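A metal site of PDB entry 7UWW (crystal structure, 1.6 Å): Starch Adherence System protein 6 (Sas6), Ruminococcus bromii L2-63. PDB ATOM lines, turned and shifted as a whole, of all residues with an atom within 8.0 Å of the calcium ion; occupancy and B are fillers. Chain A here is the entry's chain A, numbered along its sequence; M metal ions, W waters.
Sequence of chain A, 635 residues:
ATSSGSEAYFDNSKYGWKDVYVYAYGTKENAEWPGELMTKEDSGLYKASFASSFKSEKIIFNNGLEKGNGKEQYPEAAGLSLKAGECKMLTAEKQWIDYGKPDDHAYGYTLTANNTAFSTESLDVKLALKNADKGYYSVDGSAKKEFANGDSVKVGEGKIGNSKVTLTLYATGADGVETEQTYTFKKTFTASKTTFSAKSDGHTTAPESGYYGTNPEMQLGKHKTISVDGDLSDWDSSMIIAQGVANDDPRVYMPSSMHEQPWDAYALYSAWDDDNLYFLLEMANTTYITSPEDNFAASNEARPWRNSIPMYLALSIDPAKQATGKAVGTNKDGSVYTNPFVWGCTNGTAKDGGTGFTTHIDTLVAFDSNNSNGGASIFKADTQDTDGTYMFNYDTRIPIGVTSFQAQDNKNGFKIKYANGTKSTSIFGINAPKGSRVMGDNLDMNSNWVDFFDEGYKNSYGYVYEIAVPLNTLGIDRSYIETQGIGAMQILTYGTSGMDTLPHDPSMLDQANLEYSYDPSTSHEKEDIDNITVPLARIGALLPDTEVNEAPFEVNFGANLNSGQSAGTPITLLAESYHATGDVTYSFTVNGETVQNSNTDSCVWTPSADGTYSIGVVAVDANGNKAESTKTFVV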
ATOM      1  N   TYR A 212       3.338  20.030 -33.379  1.00  0.00           N
ATOM      2  CA  TYR A 212       2.255  19.802 -32.434  1.00  0.00           C
ATOM      3  C   TYR A 212       1.069  19.138 -33.133  1.00  0.00           C
ATOM      4  O   TYR A 212       0.882  19.252 -34.357  1.00  0.00           O
ATOM      5  CB  TYR A 212       1.755  21.113 -31.797  1.00  0.00           C
ATOM      6  CG  TYR A 212       2.781  21.934 -31.026  1.00  0.00           C
ATOM      7  CD1 TYR A 212       3.043  21.662 -29.682  1.00  0.00           C
ATOM      8  CD2 TYR A 212       3.467  22.970 -31.635  1.00  0.00           C
ATOM      9  CE1 TYR A 212       3.977  22.396 -28.978  1.00  0.00           C
ATOM     10  CE2 TYR A 212       4.416  23.720 -30.968  1.00  0.00           C
ATOM     11  CZ  TYR A 212       4.679  23.440 -29.635  1.00  0.00           C
ATOM     12  OH  TYR A 212       5.587  24.207 -28.967  1.00  0.00           O
ATOM     13  N   GLN A 243       0.080  15.599 -28.996  1.00  0.00           N
ATOM     14  CA  GLN A 243       1.498  15.561 -29.309  1.00  0.00           C
ATOM     15  C   GLN A 243       2.062  16.959 -29.089  1.00  0.00           C
ATOM     16  O   GLN A 243       1.621  17.935 -29.725  1.00  0.00           O
ATOM     17  CB  GLN A 243       1.707  15.065 -30.740  1.00  0.00           C
ATOM     18  CG  GLN A 243       3.167  14.972 -31.149  1.00  0.00           C
ATOM     19  CD  GLN A 243       3.927  13.998 -30.294  1.00  0.00           C
ATOM     20  OE1 GLN A 243       3.639  12.788 -30.326  1.00  0.00           O
ATOM     21  NE2 GLN A 243       4.873  14.495 -29.533  1.00  0.00           N
ATOM     22  N   GLY A 244       2.999  17.051 -28.171  1.00  0.00           N
ATOM     23  CA  GLY A 244       3.762  18.260 -27.937  1.00  0.00           C
ATOM     24  C   GLY A 244       5.107  18.216 -28.610  1.00  0.00           C
ATOM     25  O   GLY A 244       5.361  17.405 -29.514  1.00  0.00           O
ATOM     26  N   VAL A 245       5.986  19.123 -28.175  1.00  0.00           N
ATOM     27  CA  VAL A 245       7.360  19.099 -28.659  1.00  0.00           C
ATOM     28  C   VAL A 245       8.278  19.228 -27.463  1.00  0.00           C
ATOM     29  O   VAL A 245       7.877  19.616 -26.373  1.00  0.00           O
ATOM     30  CB  VAL A 245       7.690  20.213 -29.697  1.00  0.00           C
ATOM     31  CG1 VAL A 245       6.669  20.271 -30.775  1.00  0.00           C
ATOM     32  CG2 VAL A 245       7.907  21.562 -29.065  1.00  0.00           C
ATOM     33  N   ALA A 246       9.531  18.857 -27.675  1.00  0.00           N
ATOM     34  CA  ALA A 246      10.567  18.997 -26.675  1.00  0.00           C
ATOM     35  C   ALA A 246      11.210  20.381 -26.779  1.00  0.00           C
ATOM     36  O   ALA A 246      11.232  21.006 -27.861  1.00  0.00           O
ATOM     37  CB  ALA A 246      11.614  17.905 -26.826  1.00  0.00           C
ATOM     38  N   ASN A 247      11.675  20.861 -25.632  1.00  0.00           N
ATOM     39  CA  ASN A 247      12.517  22.046 -25.504  1.00  0.00           C
ATOM     40  C   ASN A 247      11.764  23.324 -25.853  1.00  0.00           C
ATOM     41  O   ASN A 247      12.360  24.305 -26.344  1.00  0.00           O
ATOM     42  CB  ASN A 247      13.784  21.923 -26.363  1.00  0.00           C
ATOM     43  CG  ASN A 247      14.945  22.715 -25.794  1.00  0.00           C
ATOM     44  OD1 ASN A 247      15.058  22.883 -24.578  1.00  0.00           O
ATOM     45  ND2 ASN A 247      15.801  23.235 -26.681  1.00  0.00           N
ATOM     46  N   ASP A 248      10.456  23.326 -25.574  1.00  0.00           N
ATOM     47  CA  ASP A 248       9.621  24.511 -25.689  1.00  0.00           C
ATOM     48  C   ASP A 248       9.059  24.955 -24.341  1.00  0.00           C
ATOM     49  O   ASP A 248       8.071  25.728 -24.297  1.00  0.00           O
ATOM     50  CB  ASP A 248       8.457  24.304 -26.660  1.00  0.00           C
ATOM     51  CG  ASP A 248       7.431  23.286 -26.156  1.00  0.00           C
ATOM     52  OD1 ASP A 248       7.777  22.522 -25.237  1.00  0.00           O
ATOM     53  OD2 ASP A 248       6.282  23.216 -26.675  1.00  0.00           O
ATOM     54  N   ASP A 249       9.635  24.505 -23.249  1.00  0.00           N
ATOM     55  CA  ASP A 249       9.243  25.013 -21.940  1.00  0.00           C
ATOM     56  C   ASP A 249       9.806  26.422 -21.755  1.00  0.00           C
ATOM     57  O   ASP A 249      10.766  26.823 -22.433  1.00  0.00           O
ATOM     58  CB  ASP A 249       9.646  24.042 -20.823  1.00  0.00           C
ATOM     59  CG  ASP A 249      11.077  23.585 -20.887  1.00  0.00           C
ATOM     60  OD1 ASP A 249      11.584  23.208 -21.975  1.00  0.00           O
ATOM     61  OD2 ASP A 249      11.661  23.533 -19.784  1.00  0.00           O
ATOM     62  N   PRO A 250       9.179  27.214 -20.906  1.00  0.00           N
ATOM     63  CA  PRO A 250       9.462  28.665 -20.916  1.00  0.00           C
ATOM     64  C   PRO A 250      10.916  29.033 -20.687  1.00  0.00           C
ATOM     65  O   PRO A 250      11.357  30.086 -21.166  1.00  0.00           O
ATOM     66  CB  PRO A 250       8.575  29.209 -19.783  1.00  0.00           C
ATOM     67  CG  PRO A 250       7.357  28.248 -19.756  1.00  0.00           C
ATOM     68  CD  PRO A 250       8.037  26.858 -20.015  1.00  0.00           C
ATOM     69  N   TRP A 263      10.314  21.703 -17.289  1.00  0.00           N
ATOM     70  CA  TRP A 263       8.931  21.229 -17.156  1.00  0.00           C
ATOM     71  C   TRP A 263       8.427  21.044 -18.588  1.00  0.00           C
ATOM     72  O   TRP A 263       7.641  21.865 -19.091  1.00  0.00           O
ATOM     73  CB  TRP A 263       8.104  22.208 -16.346  1.00  0.00           C
ATOM     74  CG  TRP A 263       8.551  22.074 -14.935  1.00  0.00           C
ATOM     75  CD1 TRP A 263       9.523  22.822 -14.291  1.00  0.00           C
ATOM     76  CD2 TRP A 263       8.165  21.072 -14.035  1.00  0.00           C
ATOM     77  NE1 TRP A 263       9.725  22.352 -13.028  1.00  0.00           N
ATOM     78  CE2 TRP A 263       8.898  21.268 -12.843  1.00  0.00           C
ATOM     79  CE3 TRP A 263       7.234  20.028 -14.097  1.00  0.00           C
ATOM     80  CZ2 TRP A 263       8.745  20.464 -11.731  1.00  0.00           C
ATOM     81  CZ3 TRP A 263       7.093  19.228 -12.979  1.00  0.00           C
ATOM     82  CH2 TRP A 263       7.844  19.449 -11.820  1.00  0.00           C
ATOM     83  N   ASP A 264       8.881  19.965 -19.220  1.00  0.00           N
ATOM     84  CA  ASP A 264       8.799  19.799 -20.671  1.00  0.00           C
ATOM     85  C   ASP A 264       7.920  18.621 -20.990  1.00  0.00           C
ATOM     86  O   ASP A 264       8.370  17.472 -21.093  1.00  0.00           O
ATOM     87  CB  ASP A 264      10.211  19.619 -21.284  1.00  0.00           C
ATOM     88  CG  ASP A 264      10.215  19.670 -22.785  1.00  0.00           C
ATOM     89  OD1 ASP A 264       9.153  19.940 -23.391  1.00  0.00           O
ATOM     90  OD2 ASP A 264      11.286  19.374 -23.399  1.00  0.00           O
ATOM     91  N   ALA A 265       6.630  18.912 -21.169  1.00  0.00           N
ATOM     92  CA  ALA A 265       5.701  17.907 -21.617  1.00  0.00           C
ATOM     93  C   ALA A 265       5.974  17.534 -23.060  1.00  0.00           C
ATOM     94  O   ALA A 265       6.202  18.404 -23.897  1.00  0.00           O
ATOM     95  CB  ALA A 265       4.278  18.454 -21.416  1.00  0.00           C
ATOM     96  N   TYR A 266       5.887  16.248 -23.377  1.00  0.00           N
ATOM     97  CA  TYR A 266       6.131  15.784 -24.740  1.00  0.00           C
ATOM     98  C   TYR A 266       4.912  15.180 -25.406  1.00  0.00           C
ATOM     99  O   TYR A 266       4.629  15.524 -26.551  1.00  0.00           O
ATOM    100  CB  TYR A 266       7.335  14.799 -24.831  1.00  0.00           C
ATOM    101  CG  TYR A 266       7.708  14.577 -26.277  1.00  0.00           C
ATOM    102  CD1 TYR A 266       8.326  15.587 -27.005  1.00  0.00           C
ATOM    103  CD2 TYR A 266       7.401  13.397 -26.934  1.00  0.00           C
ATOM    104  CE1 TYR A 266       8.600  15.433 -28.351  1.00  0.00           C
ATOM    105  CE2 TYR A 266       7.695  13.234 -28.281  1.00  0.00           C
ATOM    106  CZ  TYR A 266       8.290  14.291 -28.984  1.00  0.00           C
ATOM    107  OH  TYR A 266       8.571  14.199 -30.322  1.00  0.00           O
ATOM    108  N   ALA A 267       4.212  14.237 -24.787  1.00  0.00           N
ATOM    109  CA  ALA A 267       3.095  13.549 -25.426  1.00  0.00           C
ATOM    110  C   ALA A 267       2.169  13.042 -24.337  1.00  0.00           C
ATOM    111  O   ALA A 267       2.623  12.648 -23.263  1.00  0.00           O
ATOM    112  CB  ALA A 267       3.557  12.394 -26.335  1.00  0.00           C
ATOM    113  N   GLU A 282       4.390  11.594 -21.201  1.00  0.00           N
ATOM    114  CA  GLU A 282       5.815  11.652 -21.469  1.00  0.00           C
ATOM    115  C   GLU A 282       6.287  13.081 -21.228  1.00  0.00           C
ATOM    116  O   GLU A 282       5.714  14.015 -21.802  1.00  0.00           O
ATOM    117  CB  GLU A 282       6.138  11.272 -22.920  1.00  0.00           C
ATOM    118  CG  GLU A 282       6.188   9.819 -23.174  1.00  0.00           C
ATOM    119  CD  GLU A 282       6.686   9.506 -24.570  1.00  0.00           C
ATOM    120  OE1 GLU A 282       5.944   9.811 -25.546  1.00  0.00           O
ATOM    121  OE2 GLU A 282       7.819   9.002 -24.697  1.00  0.00           O
ATOM    122  N   MET A 283       7.332  13.240 -20.451  1.00  0.00           N
ATOM    123  CA  MET A 283       8.084  14.489 -20.299  1.00  0.00           C
ATOM    124  C   MET A 283       9.512  14.229 -20.784  1.00  0.00           C
ATOM    125  O   MET A 283      10.084  13.168 -20.529  1.00  0.00           O
ATOM    126  CB  MET A 283       8.084  14.962 -18.859  1.00  0.00           C
ATOM    127  CG  MET A 283       6.708  15.368 -18.335  1.00  0.00           C
ATOM    128  SD  MET A 283       6.651  15.626 -16.554  1.00  0.00           S
ATOM    129  CE  MET A 283       7.845  16.908 -16.341  1.00  0.00           C
ATOM    130  N   ALA A 284      10.064  15.205 -21.493  1.00  0.00           N
ATOM    131  CA  ALA A 284      11.434  15.137 -21.972  1.00  0.00           C
ATOM    132  C   ALA A 284      12.420  15.910 -21.100  1.00  0.00           C
ATOM    133  O   ALA A 284      12.067  16.837 -20.367  1.00  0.00           O
ATOM    134  CB  ALA A 284      11.508  15.647 -23.412  1.00  0.00           C
ATOM    135  N   PHE A 428      11.127  15.312 -30.988  1.00  0.00           N
ATOM    136  CA  PHE A 428      11.311  16.478 -31.850  1.00  0.00           C
ATOM    137  C   PHE A 428      11.293  17.757 -31.032  1.00  0.00           C
ATOM    138  O   PHE A 428      10.460  17.931 -30.127  1.00  0.00           O
ATOM    139  CB  PHE A 428      10.238  16.563 -32.944  1.00  0.00           C
ATOM    140  CG  PHE A 428      10.264  15.440 -33.951  1.00  0.00           C
ATOM    141  CD1 PHE A 428      11.321  15.314 -34.845  1.00  0.00           C
ATOM    142  CD2 PHE A 428       9.240  14.524 -34.009  1.00  0.00           C
ATOM    143  CE1 PHE A 428      11.347  14.266 -35.767  1.00  0.00           C
ATOM    144  CE2 PHE A 428       9.272  13.477 -34.939  1.00  0.00           C
ATOM    145  CZ  PHE A 428      10.313  13.357 -35.796  1.00  0.00           C
ATOM    146  N   LEU A 492       1.234  21.129 -16.766  1.00  0.00           N
ATOM    147  CA  LEU A 492       2.421  21.107 -15.925  1.00  0.00           C
ATOM    148  C   LEU A 492       2.647  22.511 -15.375  1.00  0.00           C
ATOM    149  O   LEU A 492       2.440  23.510 -16.075  1.00  0.00           O
ATOM    150  CB  LEU A 492       3.662  20.678 -16.707  1.00  0.00           C
ATOM    151  CG  LEU A 492       3.747  19.292 -17.303  1.00  0.00           C
ATOM    152  CD1 LEU A 492       5.130  19.072 -17.854  1.00  0.00           C
ATOM    153  CD2 LEU A 492       3.393  18.285 -16.248  1.00  0.00           C
ATOM    154  N   MET A 499       3.328  25.945 -17.118  1.00  0.00           N
ATOM    155  CA  MET A 499       4.580  25.990 -17.881  1.00  0.00           C
ATOM    156  C   MET A 499       4.483  25.330 -19.240  1.00  0.00           C
ATOM    157  O   MET A 499       5.092  25.795 -20.197  1.00  0.00           O
ATOM    158  CB  MET A 499       5.657  25.299 -17.060  1.00  0.00           C
ATOM    159  CG  MET A 499       5.961  25.984 -15.734  1.00  0.00           C
ATOM    160  SD  MET A 499       6.776  27.570 -15.922  1.00  0.00           S
ATOM    161  CE  MET A 499       8.487  26.991 -16.082  1.00  0.00           C
ATOM    162  N   ASP A 500       3.738  24.236 -19.354  1.00  0.00           N
ATOM    163  CA  ASP A 500       3.583  23.459 -20.582  1.00  0.00           C
ATOM    164  C   ASP A 500       2.242  22.744 -20.456  1.00  0.00           C
ATOM    165  O   ASP A 500       1.806  22.453 -19.345  1.00  0.00           O
ATOM    166  CB  ASP A 500       4.794  22.498 -20.759  1.00  0.00           C
ATOM    167  CG  ASP A 500       4.961  21.982 -22.180  1.00  0.00           C
ATOM    168  OD1 ASP A 500       4.075  22.195 -23.025  1.00  0.00           O
ATOM    169  OD2 ASP A 500       6.003  21.315 -22.461  1.00  0.00           O
ATOM    170  N   THR A 501       1.587  22.518 -21.585  1.00  0.00           N
ATOM    171  CA  THR A 501       0.311  21.801 -21.616  1.00  0.00           C
ATOM    172  C   THR A 501       0.285  20.850 -22.822  1.00  0.00           C
ATOM    173  O   THR A 501       0.981  21.047 -23.831  1.00  0.00           O
ATOM    174  CB  THR A 501      -0.919  22.760 -21.702  1.00  0.00           C
ATOM    175  OG1 THR A 501      -0.863  23.516 -22.927  1.00  0.00           O
ATOM    176  CG2 THR A 501      -1.016  23.711 -20.552  1.00  0.00           C
ATOM    177  N   LEU A 502      -0.549  19.816 -22.716  1.00  0.00           N
ATOM    178  CA  LEU A 502      -0.858  18.948 -23.841  1.00  0.00           C
ATOM    179  C   LEU A 502      -2.374  18.759 -23.942  1.00  0.00           C
ATOM    180  O   LEU A 502      -2.982  18.172 -23.028  1.00  0.00           O
ATOM    181  CB  LEU A 502      -0.185  17.588 -23.703  1.00  0.00           C
ATOM    182  CG  LEU A 502       1.339  17.571 -23.602  1.00  0.00           C
ATOM    183  CD1 LEU A 502       1.895  16.222 -23.195  1.00  0.00           C
ATOM    184  CD2 LEU A 502       1.929  17.987 -24.927  1.00  0.00           C
ATOM    185  N   HIS A 504      -0.783  21.679 -26.506  1.00  0.00           N
ATOM    186  CA  HIS A 504      -0.015  22.868 -26.179  1.00  0.00           C
ATOM    187  C   HIS A 504      -0.874  24.123 -26.416  1.00  0.00           C
ATOM    188  O   HIS A 504      -1.583  24.228 -27.412  1.00  0.00           O
ATOM    189  CB  HIS A 504       1.295  22.940 -27.000  1.00  0.00           C
ATOM    190  CG  HIS A 504       2.213  23.995 -26.475  1.00  0.00           C
ATOM    191  ND1 HIS A 504       2.362  25.228 -27.065  1.00  0.00           N
ATOM    192  CD2 HIS A 504       3.011  24.015 -25.387  1.00  0.00           C
ATOM    193  CE1 HIS A 504       3.210  25.964 -26.363  1.00  0.00           C
ATOM    194  NE2 HIS A 504       3.612  25.244 -25.331  1.00  0.00           N
HETATM  195 CA    CA M   1       7.094  20.473 -24.338  1.00  0.00          CA
HETATM  196  O   HOH W   1       5.099  21.069 -25.543  1.00  0.00           O
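The calcium ion is bound by O of Ala 265 (2.3 Å), OD1 of Asp 264 (2.3 Å), OD2 of Asp 500 (2.3 Å), OD1 of Asp 248 (2.3 Å), O of Val 245 (2.3 Å) and water W1 (2.4 Å).
OD2 of Asp 264 lies within hydrogen-bond range of N of Asn 247 (2.7 Å).
O of Asp 264 is in hydrogen-bond range of N of Ala 284 (2.9 Å).
The backbone carbonyl oxygen of Asp 500 is in hydrogen-bond range of the backbone NH of Leu 492, at 3.0 Å.
OD2 of Asp 248 lies within hydrogen-bond range of OH of Tyr 212, at 2.6 Å.
Water W1 lies within hydrogen-bond range of OD2 of Asp 248 (2.7 Å), OD1 of Asp 500 (2.9 Å) and N of Val 245 (3.4 Å).
Five residues have an atom within 4 Å of the calcium ion: Val 245, Asp 248, Asp 264, Ala 265 and Asp 500.
The nearest printed residue that does not touch the calcium ion is Ala 246 (4.4 Å).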
